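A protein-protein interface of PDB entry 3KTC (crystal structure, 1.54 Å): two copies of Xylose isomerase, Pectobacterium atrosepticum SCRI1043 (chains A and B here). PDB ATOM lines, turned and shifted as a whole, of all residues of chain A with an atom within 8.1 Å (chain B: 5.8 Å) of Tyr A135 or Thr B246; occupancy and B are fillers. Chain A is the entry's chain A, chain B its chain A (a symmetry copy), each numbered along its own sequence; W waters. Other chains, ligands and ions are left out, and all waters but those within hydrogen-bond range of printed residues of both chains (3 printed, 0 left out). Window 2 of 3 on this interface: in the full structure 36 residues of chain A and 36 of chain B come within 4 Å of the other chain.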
ATOM      1  N   GLY A 132     -13.571  11.283 -12.301  1.00  0.00           N
ATOM      2  CA  GLY A 132     -14.798  11.604 -12.998  1.00  0.00           C
ATOM      3  C   GLY A 132     -14.670  12.913 -13.735  1.00  0.00           C
ATOM      4  O   GLY A 132     -13.621  13.181 -14.330  1.00  0.00           O
ATOM      5  N   TRP A 133     -15.713  13.741 -13.661  1.00  0.00           N
ATOM      6  CA  TRP A 133     -15.725  15.025 -14.357  1.00  0.00           C
ATOM      7  C   TRP A 133     -16.613  15.991 -13.610  1.00  0.00           C
ATOM      8  O   TRP A 133     -17.474  15.591 -12.831  1.00  0.00           O
ATOM      9  CB  TRP A 133     -16.176  14.873 -15.826  1.00  0.00           C
ATOM     10  CG  TRP A 133     -17.514  14.203 -16.068  1.00  0.00           C
ATOM     11  CD1 TRP A 133     -17.746  12.874 -16.405  1.00  0.00           C
ATOM     12  CD2 TRP A 133     -18.829  14.807 -15.966  1.00  0.00           C
ATOM     13  NE1 TRP A 133     -19.099  12.652 -16.548  1.00  0.00           N
ATOM     14  CE2 TRP A 133     -19.778  13.813 -16.293  1.00  0.00           C
ATOM     15  CE3 TRP A 133     -19.283  16.091 -15.633  1.00  0.00           C
ATOM     16  CZ2 TRP A 133     -21.147  14.049 -16.259  1.00  0.00           C
ATOM     17  CZ3 TRP A 133     -20.654  16.339 -15.624  1.00  0.00           C
ATOM     18  CH2 TRP A 133     -21.563  15.327 -15.955  1.00  0.00           C
ATOM     19  N   ASP A 134     -16.368  17.280 -13.866  1.00  0.00           N
ATOM     20  CA  ASP A 134     -17.149  18.380 -13.321  1.00  0.00           C
ATOM     21  C   ASP A 134     -17.973  19.140 -14.359  1.00  0.00           C
ATOM     22  O   ASP A 134     -19.030  19.659 -14.029  1.00  0.00           O
ATOM     23  CB  ASP A 134     -16.217  19.323 -12.557  1.00  0.00           C
ATOM     24  CG  ASP A 134     -15.522  18.630 -11.400  1.00  0.00           C
ATOM     25  OD1 ASP A 134     -16.200  17.836 -10.686  1.00  0.00           O
ATOM     26  OD2 ASP A 134     -14.324  18.875 -11.199  1.00  0.00           O
ATOM     27  N   TYR A 135     -17.528  19.175 -15.616  1.00  0.00           N
ATOM     28  CA  TYR A 135     -18.246  19.862 -16.657  1.00  0.00           C
ATOM     29  C   TYR A 135     -18.537  19.005 -17.859  1.00  0.00           C
ATOM     30  O   TYR A 135     -17.703  18.167 -18.224  1.00  0.00           O
ATOM     31  CB  TYR A 135     -17.380  20.995 -17.175  1.00  0.00           C
ATOM     32  CG  TYR A 135     -17.146  22.125 -16.229  1.00  0.00           C
ATOM     33  CD1 TYR A 135     -16.189  22.031 -15.236  1.00  0.00           C
ATOM     34  CD2 TYR A 135     -17.873  23.284 -16.331  1.00  0.00           C
ATOM     35  CE1 TYR A 135     -15.960  23.059 -14.354  1.00  0.00           C
ATOM     36  CE2 TYR A 135     -17.654  24.325 -15.463  1.00  0.00           C
ATOM     37  CZ  TYR A 135     -16.688  24.210 -14.484  1.00  0.00           C
ATOM     38  OH  TYR A 135     -16.452  25.249 -13.625  1.00  0.00           O
ATOM     39  N   PRO A 136     -19.681  19.263 -18.529  1.00  0.00           N
ATOM     40  CA  PRO A 136     -19.814  18.700 -19.883  1.00  0.00           C
ATOM     41  C   PRO A 136     -18.615  19.098 -20.735  1.00  0.00           C
ATOM     42  O   PRO A 136     -18.093  20.197 -20.593  1.00  0.00           O
ATOM     43  CB  PRO A 136     -21.087  19.359 -20.415  1.00  0.00           C
ATOM     44  CG  PRO A 136     -21.907  19.661 -19.152  1.00  0.00           C
ATOM     45  CD  PRO A 136     -20.844  20.094 -18.163  1.00  0.00           C
ATOM     46  N   PHE A 137     -18.156  18.149 -21.553  1.00  0.00           N
ATOM     47  CA  PHE A 137     -17.019  18.305 -22.475  1.00  0.00           C
ATOM     48  C   PHE A 137     -15.628  18.290 -21.795  1.00  0.00           C
ATOM     49  O   PHE A 137     -14.618  18.333 -22.492  1.00  0.00           O
ATOM     50  CB  PHE A 137     -17.145  19.544 -23.350  1.00  0.00           C
ATOM     51  CG  PHE A 137     -18.087  19.412 -24.513  1.00  0.00           C
ATOM     52  CD1 PHE A 137     -17.661  18.802 -25.685  1.00  0.00           C
ATOM     53  CD2 PHE A 137     -19.343  20.028 -24.501  1.00  0.00           C
ATOM     54  CE1 PHE A 137     -18.458  18.769 -26.788  1.00  0.00           C
ATOM     55  CE2 PHE A 137     -20.134  19.995 -25.604  1.00  0.00           C
ATOM     56  CZ  PHE A 137     -19.692  19.367 -26.760  1.00  0.00           C
ATOM     57  N   GLN A 138     -15.552  18.189 -20.468  1.00  0.00           N
ATOM     58  CA  GLN A 138     -14.261  18.199 -19.797  1.00  0.00           C
ATOM     59  C   GLN A 138     -13.396  16.985 -20.144  1.00  0.00           C
ATOM     60  O   GLN A 138     -12.168  17.073 -20.186  1.00  0.00           O
ATOM     61  CB  GLN A 138     -14.459  18.277 -18.292  1.00  0.00           C
ATOM     62  CG  GLN A 138     -13.160  18.203 -17.519  1.00  0.00           C
ATOM     63  CD  GLN A 138     -13.341  18.505 -16.045  1.00  0.00           C
ATOM     64  OE1 GLN A 138     -14.475  18.552 -15.558  1.00  0.00           O
ATOM     65  NE2 GLN A 138     -12.227  18.783 -15.345  1.00  0.00           N
ATOM     66  N   VAL A 139     -14.054  15.868 -20.426  1.00  0.00           N
ATOM     67  CA  VAL A 139     -13.342  14.611 -20.636  1.00  0.00           C
ATOM     68  C   VAL A 139     -13.722  13.939 -21.932  1.00  0.00           C
ATOM     69  O   VAL A 139     -14.800  14.164 -22.480  1.00  0.00           O
ATOM     70  CB  VAL A 139     -13.622  13.624 -19.464  1.00  0.00           C
ATOM     71  CG1 VAL A 139     -13.137  14.201 -18.148  1.00  0.00           C
ATOM     72  CG2 VAL A 139     -15.104  13.209 -19.376  1.00  0.00           C
ATOM     73  N   HIS A 141     -15.077  10.766 -22.904  1.00  0.00           N
ATOM     74  CA  HIS A 141     -15.761   9.715 -22.135  1.00  0.00           C
ATOM     75  C   HIS A 141     -15.150   8.334 -22.377  1.00  0.00           C
ATOM     76  O   HIS A 141     -14.994   7.520 -21.441  1.00  0.00           O
ATOM     77  CB  HIS A 141     -17.253   9.752 -22.405  1.00  0.00           C
ATOM     78  CG  HIS A 141     -17.879  11.011 -21.906  1.00  0.00           C
ATOM     79  ND1 HIS A 141     -18.001  11.292 -20.565  1.00  0.00           N
ATOM     80  CD2 HIS A 141     -18.334  12.100 -22.570  1.00  0.00           C
ATOM     81  CE1 HIS A 141     -18.542  12.489 -20.426  1.00  0.00           C
ATOM     82  NE2 HIS A 141     -18.755  13.003 -21.628  1.00  0.00           N
ATOM     83  N   ARG A 174     -16.650  14.905  -7.172  1.00  0.00           N
ATOM     84  CA  ARG A 174     -16.848  15.344  -8.545  1.00  0.00           C
ATOM     85  C   ARG A 174     -18.312  15.539  -8.825  1.00  0.00           C
ATOM     86  O   ARG A 174     -19.163  15.094  -8.076  1.00  0.00           O
ATOM     87  CB  ARG A 174     -16.281  14.342  -9.555  1.00  0.00           C
ATOM     88  CG  ARG A 174     -14.816  13.950  -9.347  1.00  0.00           C
ATOM     89  CD  ARG A 174     -13.851  15.121  -9.268  1.00  0.00           C
ATOM     90  NE  ARG A 174     -13.771  15.914 -10.495  1.00  0.00           N
ATOM     91  CZ  ARG A 174     -12.973  15.666 -11.520  1.00  0.00           C
ATOM     92  NH1 ARG A 174     -12.165  14.617 -11.507  1.00  0.00           N
ATOM     93  NH2 ARG A 174     -13.004  16.482 -12.576  1.00  0.00           N
ATOM     94  N   VAL A 175     -18.629  16.204  -9.923  1.00  0.00           N
ATOM     95  CA  VAL A 175     -20.031  16.345 -10.322  1.00  0.00           C
ATOM     96  C   VAL A 175     -20.558  14.987 -10.758  1.00  0.00           C
ATOM     97  O   VAL A 175     -21.741  14.712 -10.635  1.00  0.00           O
ATOM     98  CB  VAL A 175     -20.227  17.427 -11.405  1.00  0.00           C
ATOM     99  CG1 VAL A 175     -21.675  17.458 -11.898  1.00  0.00           C
ATOM    100  CG2 VAL A 175     -19.802  18.798 -10.846  1.00  0.00           C
ATOM    101  N   LYS A 176     -19.674  14.137 -11.292  1.00  0.00           N
ATOM    102  CA  LYS A 176     -20.039  12.771 -11.683  1.00  0.00           C
ATOM    103  C   LYS A 176     -18.814  11.907 -11.486  1.00  0.00           C
ATOM    104  O   LYS A 176     -17.737  12.246 -11.958  1.00  0.00           O
ATOM    105  CB  LYS A 176     -20.475  12.718 -13.139  1.00  0.00           C
ATOM    106  CG  LYS A 176     -20.741  11.321 -13.675  1.00  0.00           C
ATOM    107  CD  LYS A 176     -21.877  10.611 -13.038  1.00  0.00           C
ATOM    108  CE  LYS A 176     -23.189  10.994 -13.635  1.00  0.00           C
ATOM    109  NZ  LYS A 176     -24.158   9.966 -13.199  1.00  0.00           N
ATOM    110  N   ASP B 233     -23.124  28.146 -12.416  1.00  0.00           N
ATOM    111  CA  ASP B 233     -23.983  27.153 -13.024  1.00  0.00           C
ATOM    112  C   ASP B 233     -23.870  25.872 -12.219  1.00  0.00           C
ATOM    113  O   ASP B 233     -22.970  25.697 -11.371  1.00  0.00           O
ATOM    114  CB  ASP B 233     -23.557  26.910 -14.482  1.00  0.00           C
ATOM    115  CG  ASP B 233     -24.737  26.625 -15.421  1.00  0.00           C
ATOM    116  OD1 ASP B 233     -25.772  26.118 -14.949  1.00  0.00           O
ATOM    117  OD2 ASP B 233     -24.610  26.903 -16.644  1.00  0.00           O
ATOM    118  N   ASP B 241     -21.560  25.201  -8.279  1.00  0.00           N
ATOM    119  CA  ASP B 241     -20.717  26.407  -8.332  1.00  0.00           C
ATOM    120  C   ASP B 241     -19.719  26.361  -9.474  1.00  0.00           C
ATOM    121  O   ASP B 241     -18.575  26.780  -9.324  1.00  0.00           O
ATOM    122  CB  ASP B 241     -20.020  26.633  -6.989  1.00  0.00           C
ATOM    123  CG  ASP B 241     -20.954  27.158  -5.925  1.00  0.00           C
ATOM    124  OD1 ASP B 241     -21.871  27.941  -6.257  1.00  0.00           O
ATOM    125  OD2 ASP B 241     -20.731  26.834  -4.747  1.00  0.00           O
ATOM    126  N   LEU B 242     -20.206  25.927 -10.631  1.00  0.00           N
ATOM    127  CA  LEU B 242     -19.453  25.858 -11.852  1.00  0.00           C
ATOM    128  C   LEU B 242     -19.444  27.231 -12.498  1.00  0.00           C
ATOM    129  O   LEU B 242     -20.258  28.086 -12.182  1.00  0.00           O
ATOM    130  CB  LEU B 242     -20.080  24.872 -12.832  1.00  0.00           C
ATOM    131  CG  LEU B 242     -20.238  23.441 -12.337  1.00  0.00           C
ATOM    132  CD1 LEU B 242     -20.986  22.629 -13.408  1.00  0.00           C
ATOM    133  CD2 LEU B 242     -18.933  22.791 -11.953  1.00  0.00           C
ATOM    134  N   VAL B 243     -18.507  27.396 -13.422  1.00  0.00           N
ATOM    135  CA  VAL B 243     -18.436  28.597 -14.266  1.00  0.00           C
ATOM    136  C   VAL B 243     -19.783  28.839 -14.976  1.00  0.00           C
ATOM    137  O   VAL B 243     -20.372  27.934 -15.577  1.00  0.00           O
ATOM    138  CB  VAL B 243     -17.291  28.488 -15.258  1.00  0.00           C
ATOM    139  CG1 VAL B 243     -17.414  29.538 -16.374  1.00  0.00           C
ATOM    140  CG2 VAL B 243     -15.927  28.594 -14.507  1.00  0.00           C
ATOM    141  N   VAL B 244     -20.268  30.064 -14.855  1.00  0.00           N
ATOM    142  CA  VAL B 244     -21.505  30.481 -15.479  1.00  0.00           C
ATOM    143  C   VAL B 244     -21.505  30.244 -16.994  1.00  0.00           C
ATOM    144  O   VAL B 244     -20.511  30.468 -17.685  1.00  0.00           O
ATOM    145  CB  VAL B 244     -21.787  31.978 -15.189  1.00  0.00           C
ATOM    146  CG1 VAL B 244     -20.709  32.847 -15.782  1.00  0.00           C
ATOM    147  CG2 VAL B 244     -23.193  32.417 -15.690  1.00  0.00           C
ATOM    148  N   GLY B 245     -22.618  29.728 -17.495  1.00  0.00           N
ATOM    149  CA  GLY B 245     -22.774  29.538 -18.923  1.00  0.00           C
ATOM    150  C   GLY B 245     -22.274  28.248 -19.505  1.00  0.00           C
ATOM    151  O   GLY B 245     -22.224  28.092 -20.707  1.00  0.00           O
ATOM    152  N   THR B 246     -21.865  27.313 -18.676  1.00  0.00           N
ATOM    153  CA  THR B 246     -21.316  26.068 -19.150  1.00  0.00           C
ATOM    154  C   THR B 246     -22.344  24.934 -19.258  1.00  0.00           C
ATOM    155  O   THR B 246     -22.027  23.892 -19.833  1.00  0.00           O
ATOM    156  CB  THR B 246     -20.159  25.629 -18.248  1.00  0.00           C
ATOM    157  OG1 THR B 246     -20.608  25.575 -16.895  1.00  0.00           O
ATOM    158  CG2 THR B 246     -18.936  26.593 -18.406  1.00  0.00           C
ATOM    159  N   VAL B 247     -23.542  25.144 -18.722  1.00  0.00           N
ATOM    160  CA  VAL B 247     -24.592  24.136 -18.714  1.00  0.00           C
ATOM    161  C   VAL B 247     -25.952  24.698 -19.145  1.00  0.00           C
ATOM    162  O   VAL B 247     -26.629  24.082 -19.965  1.00  0.00           O
ATOM    163  CB  VAL B 247     -24.733  23.423 -17.333  1.00  0.00           C
ATOM    164  CG1 VAL B 247     -25.696  22.221 -17.489  1.00  0.00           C
ATOM    165  CG2 VAL B 247     -23.357  22.949 -16.802  1.00  0.00           C
ATOM    166  N   HIS B 248     -26.344  25.844 -18.594  1.00  0.00           N
ATOM    167  CA  HIS B 248     -27.700  26.440 -18.759  1.00  0.00           C
ATOM    168  C   HIS B 248     -27.683  27.852 -19.321  1.00  0.00           C
ATOM    169  O   HIS B 248     -28.156  28.808 -18.685  1.00  0.00           O
ATOM    170  CB  HIS B 248     -28.416  26.493 -17.407  1.00  0.00           C
ATOM    171  CG  HIS B 248     -28.690  25.150 -16.831  1.00  0.00           C
ATOM    172  ND1 HIS B 248     -27.900  24.582 -15.851  1.00  0.00           N
ATOM    173  CD2 HIS B 248     -29.599  24.213 -17.172  1.00  0.00           C
ATOM    174  CE1 HIS B 248     -28.353  23.371 -15.588  1.00  0.00           C
ATOM    175  NE2 HIS B 248     -29.376  23.116 -16.383  1.00  0.00           N
ATOM    176  N   MET B 249     -27.156  27.985 -20.524  1.00  0.00           N
ATOM    177  CA  MET B 249     -27.099  29.285 -21.196  1.00  0.00           C
ATOM    178  C   MET B 249     -28.459  29.948 -21.295  1.00  0.00           C
ATOM    179  O   MET B 249     -28.631  31.126 -20.963  1.00  0.00           O
ATOM    180  CB  MET B 249     -26.502  29.139 -22.593  1.00  0.00           C
ATOM    181  CG  MET B 249     -25.026  28.893 -22.550  1.00  0.00           C
ATOM    182  SD  MET B 249     -24.573  27.030 -22.693  1.00  0.00           S
ATOM    183  CE  MET B 249     -24.712  27.094 -24.762  1.00  0.00           C
ATOM    184  N   PRO B 274     -13.881  27.196  -8.320  1.00  0.00           N
ATOM    185  CA  PRO B 274     -13.107  26.412  -9.284  1.00  0.00           C
ATOM    186  C   PRO B 274     -12.101  25.500  -8.626  1.00  0.00           C
ATOM    187  O   PRO B 274     -10.900  25.671  -8.764  1.00  0.00           O
ATOM    188  CB  PRO B 274     -12.421  27.473 -10.159  1.00  0.00           C
ATOM    189  CG  PRO B 274     -12.663  28.752  -9.515  1.00  0.00           C
ATOM    190  CD  PRO B 274     -13.471  28.609  -8.294  1.00  0.00           C
ATOM    191  N   GLU B 277      -9.436  23.911 -10.983  1.00  0.00           N
ATOM    192  CA  GLU B 277      -9.072  24.741 -12.125  1.00  0.00           C
ATOM    193  C   GLU B 277      -8.210  25.918 -11.691  1.00  0.00           C
ATOM    194  O   GLU B 277      -8.091  26.239 -10.512  1.00  0.00           O
ATOM    195  CB  GLU B 277     -10.315  25.322 -12.794  1.00  0.00           C
ATOM    196  CG  GLU B 277     -11.161  24.342 -13.613  1.00  0.00           C
ATOM    197  CD  GLU B 277     -11.856  23.284 -12.760  1.00  0.00           C
ATOM    198  OE1 GLU B 277     -12.650  23.652 -11.871  1.00  0.00           O
ATOM    199  OE2 GLU B 277     -11.550  22.095 -12.999  1.00  0.00           O
ATOM    200  N   LEU B 285     -13.069  33.318 -17.968  1.00  0.00           N
ATOM    201  CA  LEU B 285     -13.997  32.661 -18.875  1.00  0.00           C
ATOM    202  C   LEU B 285     -15.435  33.067 -18.553  1.00  0.00           C
ATOM    203  O   LEU B 285     -16.278  33.194 -19.442  1.00  0.00           O
ATOM    204  CB  LEU B 285     -13.806  31.135 -18.819  1.00  0.00           C
ATOM    205  CG  LEU B 285     -14.673  30.339 -19.815  1.00  0.00           C
ATOM    206  CD1 LEU B 285     -14.278  30.653 -21.230  1.00  0.00           C
ATOM    207  CD2 LEU B 285     -14.608  28.847 -19.517  1.00  0.00           C
ATOM    208  N   PHE B 289     -18.223  35.067 -20.992  1.00  0.00           N
ATOM    209  CA  PHE B 289     -19.566  34.619 -21.248  1.00  0.00           C
ATOM    210  C   PHE B 289     -20.589  35.690 -20.879  1.00  0.00           C
ATOM    211  O   PHE B 289     -21.573  35.917 -21.612  1.00  0.00           O
ATOM    212  CB  PHE B 289     -19.890  33.344 -20.478  1.00  0.00           C
ATOM    213  CG  PHE B 289     -21.283  32.888 -20.707  1.00  0.00           C
ATOM    214  CD1 PHE B 289     -21.611  32.204 -21.870  1.00  0.00           C
ATOM    215  CD2 PHE B 289     -22.283  33.169 -19.810  1.00  0.00           C
ATOM    216  CE1 PHE B 289     -22.917  31.797 -22.138  1.00  0.00           C
ATOM    217  CE2 PHE B 289     -23.592  32.737 -20.069  1.00  0.00           C
ATOM    218  CZ  PHE B 289     -23.888  32.041 -21.266  1.00  0.00           C
HETATM  219  O   HOH W   1     -15.121  24.582 -11.423  1.00  0.00           O
HETATM  220  O   HOH W   2     -13.262  21.756 -10.117  1.00  0.00           O
HETATM  221  O   HOH W   3     -12.311  19.730 -12.694  1.00  0.00           O
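OE1 of Gln A138 is in hydrogen-bond range of N of Tyr A135 (3.1 Å). The backbone NH of Asp A134 lies within hydrogen-bond range of the side-chain amide oxygen of Gln A138 (2.8 Å). The backbone carbonyl oxygen of Asp B233 sits at hydrogen-bond distance from the backbone NH of Leu B242, at 2.9 Å. The side-chain carboxylate (OD2) of Asp B233 lies within hydrogen-bond range of the backbone NH (N) of Thr B246 (3.4 Å). The backbone carbonyl oxygen (O) of Val B243 is in hydrogen-bond range of the side-chain hydroxyl (OG1) of Thr B246 (2.7 Å). OD1 of Asp A134 is in hydrogen-bond range of N of Val A175, 3.0 Å away.
Of the printed residues of chain B, Asp A134 touches Leu B242 (3.6 Å). Of chain B, only Leu B242, Val B243 and Thr B246 come within 4 Å of Tyr A135. Of the printed residues of chain A, Leu B242 touches Asp A134 and Tyr A135. Of chain A, only Tyr A135 (3.0 Å) comes within 4 Å of Val B243. Gly B245 touches none of the printed residues of chain A. Of chain A, only Tyr A135 (3.5 Å) comes within 4 Å of Thr B246. The nearest residue of chain B that does not touch Tyr A135 is Glu B277 (4.2 Å).
Among the printed residues, pairs that only touch across the chains: Tyr A135 with Thr B246 (3.5 Å), Tyr A135 with Leu B242 (3.5 Å) and Asp A134 with Leu B242 (3.6 Å).
Water W3 lies within hydrogen-bond range of the side-chain carboxylate (OE2) of Glu B277, the side-chain carboxylate (OD2) of Asp A134, the side-chain amide nitrogen (NE2) of Gln A138 and the guanidinium group (NH2) of Arg A174. Water W2 bridges OE1 of Glu B277 (2.7 Å) and OD2 of Asp A134 (3.3 Å). Water W1 lies within hydrogen-bond range of OH of Tyr A135 (2.7 Å) and OE1 of Glu B277 (2.7 Å).
No position is printed for both chains.
Of the 14 printed residues of chain B, 3 touch a printed residue of chain A. Printed residues of chain B that touch a printed residue of chain A: Leu B242, Val B243 and Thr B246. Hydrophobic or aromatic side chains of chain B that line the printed part of chain A: Leu B242 and Val B243. Of the 12 printed residues of chain A, 2 touch a printed residue of chain B. Among the printed residues, no Asp or Glu carboxylate lies within 4 Å of a Lys or Arg side-chain nitrogen of the other chain.
N of Val B243 is in hydrogen-bond range of OH of Tyr A135 (3.0 Å).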
